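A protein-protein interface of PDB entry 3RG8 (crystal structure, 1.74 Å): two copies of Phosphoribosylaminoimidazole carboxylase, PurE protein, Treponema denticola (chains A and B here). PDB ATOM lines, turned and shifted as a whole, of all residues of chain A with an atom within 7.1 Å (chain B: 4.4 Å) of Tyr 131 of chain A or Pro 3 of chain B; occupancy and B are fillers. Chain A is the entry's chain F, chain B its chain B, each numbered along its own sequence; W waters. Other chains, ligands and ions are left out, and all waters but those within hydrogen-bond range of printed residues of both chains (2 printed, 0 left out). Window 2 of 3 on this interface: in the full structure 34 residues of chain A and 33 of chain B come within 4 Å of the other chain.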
ATOM      1  N   ARG A 126     -11.757 -34.320 -27.221  1.00  0.00           N
ATOM      2  CA  ARG A 126     -12.726 -33.697 -26.350  1.00  0.00           C
ATOM      3  C   ARG A 126     -12.143 -33.398 -24.969  1.00  0.00           C
ATOM      4  O   ARG A 126     -12.529 -32.403 -24.367  1.00  0.00           O
ATOM      5  CB  ARG A 126     -14.023 -34.507 -26.306  1.00  0.00           C
ATOM      6  CG  ARG A 126     -14.804 -34.373 -27.580  1.00  0.00           C
ATOM      7  CD  ARG A 126     -15.960 -35.323 -27.597  1.00  0.00           C
ATOM      8  NE  ARG A 126     -17.115 -34.786 -26.863  1.00  0.00           N
ATOM      9  CZ  ARG A 126     -18.252 -35.442 -26.758  1.00  0.00           C
ATOM     10  NH1 ARG A 126     -18.365 -36.638 -27.328  1.00  0.00           N
ATOM     11  NH2 ARG A 126     -19.269 -34.930 -26.096  1.00  0.00           N
ATOM     12  N   ILE A 127     -11.154 -34.172 -24.522  1.00  0.00           N
ATOM     13  CA  ILE A 127     -10.472 -33.902 -23.276  1.00  0.00           C
ATOM     14  C   ILE A 127      -9.670 -32.591 -23.467  1.00  0.00           C
ATOM     15  O   ILE A 127      -9.775 -31.666 -22.650  1.00  0.00           O
ATOM     16  CB  ILE A 127      -9.552 -35.071 -22.843  1.00  0.00           C
ATOM     17  CG1 ILE A 127     -10.419 -36.213 -22.235  1.00  0.00           C
ATOM     18  CG2 ILE A 127      -8.491 -34.610 -21.810  1.00  0.00           C
ATOM     19  CD1 ILE A 127      -9.770 -37.597 -22.123  1.00  0.00           C
ATOM     20  N   PHE A 128      -8.886 -32.513 -24.544  1.00  0.00           N
ATOM     21  CA  PHE A 128      -8.073 -31.297 -24.783  1.00  0.00           C
ATOM     22  C   PHE A 128      -8.965 -30.095 -25.052  1.00  0.00           C
ATOM     23  O   PHE A 128      -8.611 -28.983 -24.699  1.00  0.00           O
ATOM     24  CB  PHE A 128      -7.101 -31.453 -25.947  1.00  0.00           C
ATOM     25  CG  PHE A 128      -6.067 -32.546 -25.776  1.00  0.00           C
ATOM     26  CD1 PHE A 128      -5.224 -32.579 -24.674  1.00  0.00           C
ATOM     27  CD2 PHE A 128      -5.916 -33.523 -26.742  1.00  0.00           C
ATOM     28  CE1 PHE A 128      -4.267 -33.569 -24.543  1.00  0.00           C
ATOM     29  CE2 PHE A 128      -4.957 -34.505 -26.633  1.00  0.00           C
ATOM     30  CZ  PHE A 128      -4.139 -34.550 -25.525  1.00  0.00           C
ATOM     31  N   SER A 129     -10.128 -30.323 -25.681  1.00  0.00           N
ATOM     32  CA  SER A 129     -11.066 -29.253 -26.053  1.00  0.00           C
ATOM     33  C   SER A 129     -11.541 -28.400 -24.864  1.00  0.00           C
ATOM     34  O   SER A 129     -11.907 -27.260 -25.070  1.00  0.00           O
ATOM     35  CB  SER A 129     -12.291 -29.807 -26.801  1.00  0.00           C
ATOM     36  OG  SER A 129     -13.312 -30.189 -25.922  1.00  0.00           O
ATOM     37  N   LEU A 130     -11.449 -28.894 -23.625  1.00  0.00           N
ATOM     38  CA  LEU A 130     -11.816 -28.060 -22.458  1.00  0.00           C
ATOM     39  C   LEU A 130     -10.989 -26.769 -22.325  1.00  0.00           C
ATOM     40  O   LEU A 130     -11.470 -25.789 -21.726  1.00  0.00           O
ATOM     41  CB  LEU A 130     -11.683 -28.853 -21.154  1.00  0.00           C
ATOM     42  CG  LEU A 130     -12.501 -30.138 -21.003  1.00  0.00           C
ATOM     43  CD1 LEU A 130     -12.682 -30.507 -19.501  1.00  0.00           C
ATOM     44  CD2 LEU A 130     -13.801 -30.131 -21.817  1.00  0.00           C
ATOM     45  N   TYR A 131      -9.741 -26.813 -22.815  1.00  0.00           N
ATOM     46  CA  TYR A 131      -8.782 -25.728 -22.738  1.00  0.00           C
ATOM     47  C   TYR A 131      -8.163 -25.305 -24.124  1.00  0.00           C
ATOM     48  O   TYR A 131      -7.534 -24.232 -24.221  1.00  0.00           O
ATOM     49  CB  TYR A 131      -7.664 -26.154 -21.748  1.00  0.00           C
ATOM     50  CG  TYR A 131      -8.092 -26.406 -20.290  1.00  0.00           C
ATOM     51  CD1 TYR A 131      -8.015 -25.395 -19.329  1.00  0.00           C
ATOM     52  CD2 TYR A 131      -8.545 -27.665 -19.867  1.00  0.00           C
ATOM     53  CE1 TYR A 131      -8.364 -25.615 -17.998  1.00  0.00           C
ATOM     54  CE2 TYR A 131      -8.921 -27.894 -18.536  1.00  0.00           C
ATOM     55  CZ  TYR A 131      -8.835 -26.861 -17.609  1.00  0.00           C
ATOM     56  OH  TYR A 131      -9.159 -27.065 -16.292  1.00  0.00           O
ATOM     57  N   ASP A 132      -8.383 -26.090 -25.196  1.00  0.00           N
ATOM     58  CA  ASP A 132      -7.747 -25.839 -26.488  1.00  0.00           C
ATOM     59  C   ASP A 132      -8.881 -25.529 -27.450  1.00  0.00           C
ATOM     60  O   ASP A 132      -9.591 -26.463 -27.857  1.00  0.00           O
ATOM     61  CB  ASP A 132      -6.928 -27.067 -26.952  1.00  0.00           C
ATOM     62  CG  ASP A 132      -6.069 -26.775 -28.159  1.00  0.00           C
ATOM     63  OD1 ASP A 132      -6.594 -26.261 -29.177  1.00  0.00           O
ATOM     64  OD2 ASP A 132      -4.841 -27.040 -28.111  1.00  0.00           O
ATOM     65  N   LYS A 133      -9.093 -24.245 -27.750  1.00  0.00           N
ATOM     66  CA  LYS A 133     -10.225 -23.834 -28.562  1.00  0.00           C
ATOM     67  C   LYS A 133     -10.096 -24.279 -30.020  1.00  0.00           C
ATOM     68  O   LYS A 133     -11.117 -24.537 -30.653  1.00  0.00           O
ATOM     69  CB  LYS A 133     -10.514 -22.317 -28.496  1.00  0.00           C
ATOM     70  CG  LYS A 133     -11.788 -21.997 -29.286  1.00  0.00           C
ATOM     71  CD  LYS A 133     -12.497 -20.727 -28.904  1.00  0.00           C
ATOM     72  CE  LYS A 133     -13.656 -20.927 -27.939  1.00  0.00           C
ATOM     73  NZ  LYS A 133     -14.054 -19.607 -27.396  1.00  0.00           N
ATOM     74  N   GLU A 134      -8.882 -24.419 -30.548  1.00  0.00           N
ATOM     75  CA  GLU A 134      -8.711 -24.948 -31.913  1.00  0.00           C
ATOM     76  C   GLU A 134      -9.263 -26.382 -31.979  1.00  0.00           C
ATOM     77  O   GLU A 134     -10.056 -26.744 -32.846  1.00  0.00           O
ATOM     78  CB  GLU A 134      -7.228 -24.942 -32.344  1.00  0.00           C
ATOM     79  CG  GLU A 134      -7.001 -24.765 -33.855  1.00  0.00           C
ATOM     80  CD  GLU A 134      -5.523 -24.838 -34.262  1.00  0.00           C
ATOM     81  OE1 GLU A 134      -4.735 -23.955 -33.859  1.00  0.00           O
ATOM     82  OE2 GLU A 134      -5.147 -25.773 -35.006  1.00  0.00           O
ATOM     83  N   ALA A 136     -11.411 -27.646 -29.936  1.00  0.00           N
ATOM     84  CA  ALA A 136     -12.868 -27.616 -29.744  1.00  0.00           C
ATOM     85  C   ALA A 136     -13.589 -27.277 -31.035  1.00  0.00           C
ATOM     86  O   ALA A 136     -14.699 -27.750 -31.278  1.00  0.00           O
ATOM     87  CB  ALA A 136     -13.280 -26.632 -28.671  1.00  0.00           C
ATOM     88  N   ARG B   2     -10.914 -23.016 -12.279  1.00  0.00           N
ATOM     89  CA  ARG B   2     -12.383 -22.923 -12.218  1.00  0.00           C
ATOM     90  C   ARG B   2     -13.092 -24.076 -12.961  1.00  0.00           C
ATOM     91  O   ARG B   2     -14.081 -23.837 -13.646  1.00  0.00           O
ATOM     92  CB  ARG B   2     -12.815 -21.602 -12.823  1.00  0.00           C
ATOM     93  CG  ARG B   2     -14.242 -21.177 -12.409  1.00  0.00           C
ATOM     94  CD  ARG B   2     -14.927 -20.286 -13.456  1.00  0.00           C
ATOM     95  NE  ARG B   2     -14.093 -19.133 -13.777  1.00  0.00           N
ATOM     96  CZ  ARG B   2     -13.288 -19.011 -14.840  1.00  0.00           C
ATOM     97  NH1 ARG B   2     -13.173 -19.974 -15.763  1.00  0.00           N
ATOM     98  NH2 ARG B   2     -12.578 -17.893 -14.982  1.00  0.00           N
ATOM     99  N   PRO B   3     -12.557 -25.307 -12.875  1.00  0.00           N
ATOM    100  CA  PRO B   3     -13.276 -26.462 -13.441  1.00  0.00           C
ATOM    101  C   PRO B   3     -14.633 -26.706 -12.787  1.00  0.00           C
ATOM    102  O   PRO B   3     -14.851 -26.288 -11.658  1.00  0.00           O
ATOM    103  CB  PRO B   3     -12.332 -27.616 -13.167  1.00  0.00           C
ATOM    104  CG  PRO B   3     -10.949 -26.945 -13.148  1.00  0.00           C
ATOM    105  CD  PRO B   3     -11.160 -25.651 -12.548  1.00  0.00           C
ATOM    106  N   LEU B   4     -15.551 -27.324 -13.536  1.00  0.00           N
ATOM    107  CA  LEU B   4     -16.864 -27.707 -13.015  1.00  0.00           C
ATOM    108  C   LEU B   4     -17.128 -29.135 -13.474  1.00  0.00           C
ATOM    109  O   LEU B   4     -16.924 -29.440 -14.658  1.00  0.00           O
ATOM    110  CB  LEU B   4     -17.988 -26.815 -13.553  1.00  0.00           C
ATOM    111  CG  LEU B   4     -19.412 -27.148 -13.097  1.00  0.00           C
ATOM    112  CD1 LEU B   4     -19.513 -27.126 -11.571  1.00  0.00           C
ATOM    113  CD2 LEU B   4     -20.422 -26.248 -13.715  1.00  0.00           C
ATOM    114  N   GLU B  31     -15.091 -28.222  -7.844  1.00  0.00           N
ATOM    115  CA  GLU B  31     -16.511 -27.874  -7.753  1.00  0.00           C
ATOM    116  C   GLU B  31     -17.371 -28.871  -8.551  1.00  0.00           C
ATOM    117  O   GLU B  31     -17.029 -29.247  -9.692  1.00  0.00           O
ATOM    118  CB  GLU B  31     -16.767 -26.459  -8.302  1.00  0.00           C
ATOM    119  CG  GLU B  31     -18.171 -25.932  -8.078  1.00  0.00           C
ATOM    120  CD  GLU B  31     -18.387 -24.471  -8.555  1.00  0.00           C
ATOM    121  OE1 GLU B  31     -17.427 -23.671  -8.614  1.00  0.00           O
ATOM    122  OE2 GLU B  31     -19.543 -24.124  -8.884  1.00  0.00           O
ATOM    123  N   ARG B  58     -16.335 -21.929 -18.773  1.00  0.00           N
ATOM    124  CA  ARG B  58     -15.381 -22.546 -17.839  1.00  0.00           C
ATOM    125  C   ARG B  58     -15.152 -24.010 -18.264  1.00  0.00           C
ATOM    126  O   ARG B  58     -16.006 -24.601 -18.900  1.00  0.00           O
ATOM    127  CB  ARG B  58     -15.898 -22.522 -16.398  1.00  0.00           C
ATOM    128  CG  ARG B  58     -17.142 -23.358 -16.150  1.00  0.00           C
ATOM    129  CD  ARG B  58     -17.866 -22.972 -14.869  1.00  0.00           C
ATOM    130  NE  ARG B  58     -17.061 -23.329 -13.725  1.00  0.00           N
ATOM    131  CZ  ARG B  58     -17.467 -23.328 -12.462  1.00  0.00           C
ATOM    132  NH1 ARG B  58     -18.691 -22.928 -12.125  1.00  0.00           N
ATOM    133  NH2 ARG B  58     -16.637 -23.741 -11.528  1.00  0.00           N
ATOM    134  N   PRO B  59     -14.002 -24.593 -17.909  1.00  0.00           N
ATOM    135  CA  PRO B  59     -13.813 -25.993 -18.298  1.00  0.00           C
ATOM    136  C   PRO B  59     -14.723 -26.930 -17.493  1.00  0.00           C
ATOM    137  O   PRO B  59     -14.842 -26.795 -16.263  1.00  0.00           O
ATOM    138  CB  PRO B  59     -12.342 -26.243 -18.042  1.00  0.00           C
ATOM    139  CG  PRO B  59     -11.932 -25.176 -17.018  1.00  0.00           C
ATOM    140  CD  PRO B  59     -12.953 -24.107 -16.998  1.00  0.00           C
ATOM    141  N   PHE B 128      -8.662 -32.671 -15.915  1.00  0.00           N
ATOM    142  CA  PHE B 128      -8.391 -31.279 -15.694  1.00  0.00           C
ATOM    143  C   PHE B 128      -6.899 -31.055 -15.486  1.00  0.00           C
ATOM    144  O   PHE B 128      -6.365 -29.977 -15.779  1.00  0.00           O
ATOM    145  CB  PHE B 128      -9.162 -30.692 -14.500  1.00  0.00           C
ATOM    146  CG  PHE B 128     -10.669 -30.697 -14.675  1.00  0.00           C
ATOM    147  CD1 PHE B 128     -11.249 -30.152 -15.807  1.00  0.00           C
ATOM    148  CD2 PHE B 128     -11.490 -31.268 -13.690  1.00  0.00           C
ATOM    149  CE1 PHE B 128     -12.659 -30.143 -15.957  1.00  0.00           C
ATOM    150  CE2 PHE B 128     -12.859 -31.288 -13.805  1.00  0.00           C
ATOM    151  CZ  PHE B 128     -13.463 -30.739 -14.967  1.00  0.00           C
ATOM    152  N   TYR B 131      -4.102 -29.311 -17.721  1.00  0.00           N
ATOM    153  CA  TYR B 131      -4.015 -27.871 -17.779  1.00  0.00           C
ATOM    154  C   TYR B 131      -4.126 -27.159 -16.423  1.00  0.00           C
ATOM    155  O   TYR B 131      -3.953 -25.962 -16.396  1.00  0.00           O
ATOM    156  CB  TYR B 131      -5.105 -27.313 -18.706  1.00  0.00           C
ATOM    157  CG  TYR B 131      -4.971 -27.740 -20.129  1.00  0.00           C
ATOM    158  CD1 TYR B 131      -5.553 -28.931 -20.563  1.00  0.00           C
ATOM    159  CD2 TYR B 131      -4.227 -26.992 -21.045  1.00  0.00           C
ATOM    160  CE1 TYR B 131      -5.439 -29.347 -21.862  1.00  0.00           C
ATOM    161  CE2 TYR B 131      -4.093 -27.408 -22.377  1.00  0.00           C
ATOM    162  CZ  TYR B 131      -4.728 -28.597 -22.774  1.00  0.00           C
ATOM    163  OH  TYR B 131      -4.631 -29.036 -24.075  1.00  0.00           O
ATOM    164  N   ASP B 132      -4.357 -27.885 -15.323  1.00  0.00           N
ATOM    165  CA  ASP B 132      -4.693 -27.250 -14.043  1.00  0.00           C
ATOM    166  C   ASP B 132      -3.722 -27.822 -13.005  1.00  0.00           C
ATOM    167  O   ASP B 132      -3.862 -28.965 -12.564  1.00  0.00           O
ATOM    168  CB  ASP B 132      -6.142 -27.460 -13.616  1.00  0.00           C
ATOM    169  CG  ASP B 132      -6.503 -26.693 -12.320  1.00  0.00           C
ATOM    170  OD1 ASP B 132      -5.742 -26.730 -11.333  1.00  0.00           O
ATOM    171  OD2 ASP B 132      -7.557 -26.041 -12.300  1.00  0.00           O
ATOM    172  N   ILE B 135      -4.876 -29.142  -9.354  1.00  0.00           N
ATOM    173  CA  ILE B 135      -5.519 -30.467  -9.459  1.00  0.00           C
ATOM    174  C   ILE B 135      -4.432 -31.517  -9.758  1.00  0.00           C
ATOM    175  O   ILE B 135      -4.436 -32.616  -9.204  1.00  0.00           O
ATOM    176  CB  ILE B 135      -6.608 -30.441 -10.534  1.00  0.00           C
ATOM    177  CG1 ILE B 135      -7.765 -29.542 -10.108  1.00  0.00           C
ATOM    178  CG2 ILE B 135      -7.240 -31.875 -10.808  1.00  0.00           C
ATOM    179  CD1 ILE B 135      -8.669 -29.183 -11.268  1.00  0.00           C
HETATM  180  O   HOH W   1      -3.725 -27.169 -25.841  1.00  0.00           O
HETATM  181  O   HOH W   2      -8.465 -24.992 -14.730  1.00  0.00           O
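N of Leu 4 of chain B lies within hydrogen-bond range of O of Pro 59 of chain B. The backbone carbonyl oxygen of Pro 3 of chain B is in hydrogen-bond range of the guanidinium group of Arg 58 of chain B (3.1 Å).
CD1 of Phe 128 of chain A touches OH of Tyr 131 of chain B (3.6 Å). Pro 59 of chain B touches Leu 130 of chain A. CE1 of Phe 128 of chain B touches CD1 of Leu 130 of chain A, 3.6 Å away. Pro 3 of chain B touches Tyr 131 of chain A. OH of Tyr 131 of chain A touches CG of Pro 59 of chain B, 3.4 Å away. Tyr 131 of chain A touches Phe 128 of chain B. CD2 of Tyr 131 of chain A touches CD1 of Tyr 131 of chain B, at 3.3 Å.
Printed residues of chain B within 4 Å of Phe 128 of chain A: Tyr 131. Of the printed residues of chain B, Leu 130 of chain A touches Pro 59 and Phe 128. Of the printed residues of chain B, Tyr 131 of chain A touches Pro 3, Pro 59, Phe 128 and Tyr 131. Pro 3 of chain B touches just one residue of chain A: Tyr 131 (3.6 Å). Of the printed residues of chain A, Pro 59 of chain B touches Leu 130 and Tyr 131. Of the printed residues of chain A, Tyr 131 of chain B touches Phe 128 and Tyr 131.
Printed residues of chain B that touch a printed residue of chain A: Pro 3, Pro 59, Phe 128 and Tyr 131. Printed residues of chain A that touch a printed residue of chain B: Phe 128, Leu 130 and Tyr 131. Hydrophobic or aromatic side chains of chain A within 4 Å of the printed part of chain B: Phe 128, Leu 130 and Tyr 131.
Phe 128 of chain A touches Tyr 131 of chain B, and with the chains exchanged Tyr 131 of chain A touches Phe 128 of chain B. Tyr 131 of chain B touches its own counterpart, Tyr 131 of chain A. Positions printed for both chains: 128, 131 and 132.
Water W1 lies within hydrogen-bond range of the side-chain carboxylate (OD2) of Asp 132 of chain A and the side-chain hydroxyl (OH) of Tyr 131 of chain B. Water W2 bridges the side-chain hydroxyl (OH) of Tyr 131 of chain A (2.7 Å) and the side-chain carboxylate (OD2) of Asp 132 of chain B (2.8 Å).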
